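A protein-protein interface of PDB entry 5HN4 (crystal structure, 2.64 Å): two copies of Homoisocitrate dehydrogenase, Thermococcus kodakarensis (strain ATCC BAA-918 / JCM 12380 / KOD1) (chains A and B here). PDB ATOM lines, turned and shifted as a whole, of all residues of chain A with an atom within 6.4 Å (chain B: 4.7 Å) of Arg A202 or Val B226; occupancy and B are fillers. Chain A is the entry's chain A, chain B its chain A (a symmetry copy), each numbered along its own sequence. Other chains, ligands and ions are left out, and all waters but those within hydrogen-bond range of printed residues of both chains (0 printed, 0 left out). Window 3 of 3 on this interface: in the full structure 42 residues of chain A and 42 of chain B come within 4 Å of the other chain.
Arg A202 touches just one residue of chain B: Val B226 (2.7 Å). Of chain A, only Val A201 (3.7 Å) and Arg A202 (2.7 Å) come within 4 Å of Val B226. Printed residues of chain B within 4 Å of Val A201: Leu B223 (3.7 Å) and Val B226 (3.7 Å). Of the printed residues of chain B, Ile A198 touches Asp B222 and Thr B225. Of the printed residues of chain B, Thr A197 touches Asp B222 and Leu B223. Printed residues of chain A within 4 Å of Leu B223: Thr A197 and Val A201. Printed residues of chain A within 4 Å of Thr B225: Ile A198. Leu A200 touches none of the printed residues of chain B. The nearest residue of chain A that does not touch Val B226 is Ile A198 (4.3 Å).
Position printed for both chains: 227.
Of the 7 printed residues of chain B, 4 touch a printed residue of chain A. Hydrophobic or aromatic side chains of chain B within 4 Å of the printed part of chain A: Leu B223 and Val B226. Of the 9 printed residues of chain A, 4 touch a printed residue of chain B. Along chain A the printed residues that touch a printed residue of chain B span positions 197 to 202. Among the printed residues, 7 pairs touch across the chains. Among the printed residues, no Asp or Glu carboxylate lies within 4 Å of a Lys or Arg side-chain nitrogen of the other chain.
The backbone carbonyl oxygen of Asp B222 lies within hydrogen-bond range of the side-chain hydroxyl of Thr B225 (2.7 Å).
OG1 of Thr A197 touches C of Asp B222 (3.9 Å). Asp B222 touches Ile A198. Thr B225 touches Ile A198. Val A201 touches Leu B223. Val B226 touches Val A201 (CG1 to CG2, 3.7 Å).
The guanidinium group (NH2) of Arg A202 is in hydrogen-bond range of the backbone carbonyl oxygen (O) of Val B226 (2.7 Å). The side-chain hydroxyl of Thr A197 lies close to the backbone NH of Leu B223 (3.3 Å).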
ATOM      1  N   THR A 197      -4.693  -7.284  -0.047  1.00  0.00           N
ATOM      2  CA  THR A 197      -5.322  -6.722  -1.207  1.00  0.00           C
ATOM      3  C   THR A 197      -5.951  -7.834  -2.033  1.00  0.00           C
ATOM      4  O   THR A 197      -7.011  -7.645  -2.550  1.00  0.00           O
ATOM      5  CB  THR A 197      -4.375  -5.923  -2.094  1.00  0.00           C
ATOM      6  OG1 THR A 197      -3.388  -6.792  -2.668  1.00  0.00           O
ATOM      7  CG2 THR A 197      -3.730  -4.781  -1.289  1.00  0.00           C
ATOM      8  N   ILE A 198      -5.307  -8.996  -2.114  1.00  0.00           N
ATOM      9  CA  ILE A 198      -5.839 -10.118  -2.874  1.00  0.00           C
ATOM     10  C   ILE A 198      -7.109 -10.627  -2.187  1.00  0.00           C
ATOM     11  O   ILE A 198      -8.161 -10.781  -2.822  1.00  0.00           O
ATOM     12  CB  ILE A 198      -4.781 -11.250  -3.016  1.00  0.00           C
ATOM     13  CG1 ILE A 198      -3.651 -10.830  -3.977  1.00  0.00           C
ATOM     14  CG2 ILE A 198      -5.415 -12.547  -3.510  1.00  0.00           C
ATOM     15  CD1 ILE A 198      -2.326 -11.568  -3.737  1.00  0.00           C
ATOM     16  N   LYS A 199      -7.014 -10.855  -0.882  1.00  0.00           N
ATOM     17  CA  LYS A 199      -8.183 -11.256  -0.105  1.00  0.00           C
ATOM     18  C   LYS A 199      -9.369 -10.292  -0.239  1.00  0.00           C
ATOM     19  O   LYS A 199     -10.517 -10.710  -0.163  1.00  0.00           O
ATOM     20  CB  LYS A 199      -7.825 -11.403   1.368  1.00  0.00           C
ATOM     21  CG  LYS A 199      -6.889 -12.565   1.685  1.00  0.00           C
ATOM     22  CD  LYS A 199      -6.774 -12.749   3.183  1.00  0.00           C
ATOM     23  CE  LYS A 199      -5.833 -13.876   3.559  1.00  0.00           C
ATOM     24  NZ  LYS A 199      -4.424 -13.498   3.291  1.00  0.00           N
ATOM     25  N   LEU A 200      -9.089  -9.005  -0.419  1.00  0.00           N
ATOM     26  CA  LEU A 200     -10.132  -8.002  -0.426  1.00  0.00           C
ATOM     27  C   LEU A 200     -10.867  -8.037  -1.745  1.00  0.00           C
ATOM     28  O   LEU A 200     -12.080  -7.877  -1.759  1.00  0.00           O
ATOM     29  CB  LEU A 200      -9.561  -6.593  -0.163  1.00  0.00           C
ATOM     30  CG  LEU A 200     -10.569  -5.431  -0.094  1.00  0.00           C
ATOM     31  CD1 LEU A 200     -11.722  -5.768   0.839  1.00  0.00           C
ATOM     32  CD2 LEU A 200      -9.920  -4.142   0.357  1.00  0.00           C
ATOM     33  N   VAL A 201     -10.162  -8.232  -2.858  1.00  0.00           N
ATOM     34  CA  VAL A 201     -10.902  -8.351  -4.115  1.00  0.00           C
ATOM     35  C   VAL A 201     -11.576  -9.730  -4.297  1.00  0.00           C
ATOM     36  O   VAL A 201     -12.572  -9.813  -4.955  1.00  0.00           O
ATOM     37  CB  VAL A 201     -10.160  -7.879  -5.392  1.00  0.00           C
ATOM     38  CG1 VAL A 201      -8.908  -7.089  -5.092  1.00  0.00           C
ATOM     39  CG2 VAL A 201      -9.926  -8.998  -6.365  1.00  0.00           C
ATOM     40  N   ARG A 202     -11.076 -10.777  -3.664  1.00  0.00           N
ATOM     41  CA  ARG A 202     -11.566 -12.122  -3.909  1.00  0.00           C
ATOM     42  C   ARG A 202     -12.613 -12.578  -2.929  1.00  0.00           C
ATOM     43  O   ARG A 202     -13.547 -13.272  -3.297  1.00  0.00           O
ATOM     44  CB  ARG A 202     -10.412 -13.117  -3.885  1.00  0.00           C
ATOM     45  CG  ARG A 202      -9.509 -12.948  -5.086  1.00  0.00           C
ATOM     46  CD  ARG A 202      -9.327 -14.216  -5.895  1.00  0.00           C
ATOM     47  NE  ARG A 202      -8.999 -13.866  -7.281  1.00  0.00           N
ATOM     48  CZ  ARG A 202      -7.846 -14.118  -7.900  1.00  0.00           C
ATOM     49  NH1 ARG A 202      -6.855 -14.765  -7.289  1.00  0.00           N
ATOM     50  NH2 ARG A 202      -7.695 -13.731  -9.161  1.00  0.00           N
ATOM     51  N   ASN A 203     -12.457 -12.197  -1.681  1.00  0.00           N
ATOM     52  CA  ASN A 203     -13.349 -12.634  -0.667  1.00  0.00           C
ATOM     53  C   ASN A 203     -13.825 -11.422   0.134  1.00  0.00           C
ATOM     54  O   ASN A 203     -13.579 -11.314   1.341  1.00  0.00           O
ATOM     55  CB  ASN A 203     -12.610 -13.645   0.189  1.00  0.00           C
ATOM     56  CG  ASN A 203     -13.494 -14.278   1.250  1.00  0.00           C
ATOM     57  OD1 ASN A 203     -14.710 -14.404   1.067  1.00  0.00           O
ATOM     58  ND2 ASN A 203     -12.892 -14.657   2.383  1.00  0.00           N
ATOM     59  N   PRO A 204     -14.542 -10.509  -0.529  1.00  0.00           N
ATOM     60  CA  PRO A 204     -14.869  -9.218   0.076  1.00  0.00           C
ATOM     61  C   PRO A 204     -15.618  -9.208   1.394  1.00  0.00           C
ATOM     62  O   PRO A 204     -15.367  -8.327   2.225  1.00  0.00           O
ATOM     63  CB  PRO A 204     -15.724  -8.524  -0.981  1.00  0.00           C
ATOM     64  CG  PRO A 204     -16.035  -9.559  -2.017  1.00  0.00           C
ATOM     65  CD  PRO A 204     -14.913 -10.553  -1.949  1.00  0.00           C
ATOM     66  N   HIS A 227     -16.210  -3.392  -5.230  1.00  0.00           N
ATOM     67  CA  HIS A 227     -17.327  -4.286  -5.004  1.00  0.00           C
ATOM     68  C   HIS A 227     -18.691  -3.603  -4.996  1.00  0.00           C
ATOM     69  O   HIS A 227     -19.668  -4.194  -4.538  1.00  0.00           O
ATOM     70  CB  HIS A 227     -17.133  -5.037  -3.699  1.00  0.00           C
ATOM     71  CG  HIS A 227     -15.895  -5.867  -3.677  1.00  0.00           C
ATOM     72  ND1 HIS A 227     -15.649  -6.849  -4.603  1.00  0.00           N
ATOM     73  CD2 HIS A 227     -14.831  -5.858  -2.847  1.00  0.00           C
ATOM     74  CE1 HIS A 227     -14.487  -7.415  -4.348  1.00  0.00           C
ATOM     75  NE2 HIS A 227     -13.969  -6.828  -3.285  1.00  0.00           N
ATOM     76  N   ASP B 222       1.284  -7.342  -5.308  1.00  0.00           N
ATOM     77  CA  ASP B 222       0.346  -8.376  -4.879  1.00  0.00           C
ATOM     78  C   ASP B 222      -1.037  -8.153  -5.467  1.00  0.00           C
ATOM     79  O   ASP B 222      -1.620  -9.089  -5.993  1.00  0.00           O
ATOM     80  CB  ASP B 222       0.222  -8.469  -3.382  1.00  0.00           C
ATOM     81  CG  ASP B 222       1.124  -9.515  -2.793  1.00  0.00           C
ATOM     82  OD1 ASP B 222       2.249  -9.716  -3.287  1.00  0.00           O
ATOM     83  OD2 ASP B 222       0.698 -10.124  -1.802  1.00  0.00           O
ATOM     84  N   LEU B 223      -1.543  -6.919  -5.423  1.00  0.00           N
ATOM     85  CA  LEU B 223      -2.873  -6.635  -5.942  1.00  0.00           C
ATOM     86  C   LEU B 223      -3.009  -7.036  -7.418  1.00  0.00           C
ATOM     87  O   LEU B 223      -4.025  -7.581  -7.810  1.00  0.00           O
ATOM     88  CB  LEU B 223      -3.208  -5.153  -5.807  1.00  0.00           C
ATOM     89  CG  LEU B 223      -4.536  -4.721  -6.455  1.00  0.00           C
ATOM     90  CD1 LEU B 223      -5.677  -5.565  -5.922  1.00  0.00           C
ATOM     91  CD2 LEU B 223      -4.864  -3.271  -6.203  1.00  0.00           C
ATOM     92  N   ALA B 224      -1.974  -6.754  -8.210  1.00  0.00           N
ATOM     93  CA  ALA B 224      -1.948  -7.056  -9.630  1.00  0.00           C
ATOM     94  C   ALA B 224      -2.030  -8.543  -9.923  1.00  0.00           C
ATOM     95  O   ALA B 224      -2.405  -8.931 -11.021  1.00  0.00           O
ATOM     96  CB  ALA B 224      -0.677  -6.510 -10.266  1.00  0.00           C
ATOM     97  N   THR B 225      -1.675  -9.382  -8.954  1.00  0.00           N
ATOM     98  CA  THR B 225      -1.719 -10.799  -9.207  1.00  0.00           C
ATOM     99  C   THR B 225      -3.133 -11.323  -9.360  1.00  0.00           C
ATOM    100  O   THR B 225      -3.304 -12.413  -9.900  1.00  0.00           O
ATOM    101  CB  THR B 225      -1.032 -11.628  -8.124  1.00  0.00           C
ATOM    102  OG1 THR B 225      -1.805 -11.592  -6.911  1.00  0.00           O
ATOM    103  CG2 THR B 225       0.451 -11.180  -7.938  1.00  0.00           C
ATOM    104  N   VAL B 226      -4.148 -10.578  -8.916  1.00  0.00           N
ATOM    105  CA  VAL B 226      -5.510 -11.050  -9.141  1.00  0.00           C
ATOM    106  C   VAL B 226      -5.783 -11.266 -10.624  1.00  0.00           C
ATOM    107  O   VAL B 226      -6.635 -12.034 -10.941  1.00  0.00           O
ATOM    108  CB  VAL B 226      -6.604 -10.134  -8.583  1.00  0.00           C
ATOM    109  CG1 VAL B 226      -6.442 -10.019  -7.088  1.00  0.00           C
ATOM    110  CG2 VAL B 226      -6.633  -8.777  -9.298  1.00  0.00           C
ATOM    111  N   HIS B 227      -5.048 -10.621 -11.526  1.00  0.00           N
ATOM    112  CA  HIS B 227      -5.301 -10.809 -12.940  1.00  0.00           C
ATOM    113  C   HIS B 227      -4.626 -12.036 -13.545  1.00  0.00           C
ATOM    114  O   HIS B 227      -4.531 -12.141 -14.768  1.00  0.00           O
ATOM    115  CB  HIS B 227      -4.878  -9.571 -13.711  1.00  0.00           C
ATOM    116  CG  HIS B 227      -5.609  -8.341 -13.292  1.00  0.00           C
ATOM    117  ND1 HIS B 227      -6.977  -8.245 -13.339  1.00  0.00           N
ATOM    118  CD2 HIS B 227      -5.164  -7.159 -12.815  1.00  0.00           C
ATOM    119  CE1 HIS B 227      -7.350  -7.056 -12.910  1.00  0.00           C
ATOM    120  NE2 HIS B 227      -6.266  -6.378 -12.584  1.00  0.00           N
ATOM    121  N   ALA B 228      -4.153 -12.964 -12.721  1.00  0.00           N
ATOM    122  CA  ALA B 228      -3.442 -14.129 -13.248  1.00  0.00           C
ATOM    123  C   ALA B 228      -4.098 -15.355 -12.696  1.00  0.00           C
ATOM    124  O   ALA B 228      -4.904 -15.262 -11.781  1.00  0.00           O
ATOM    125  CB  ALA B 228      -1.982 -14.090 -12.863  1.00  0.00           C
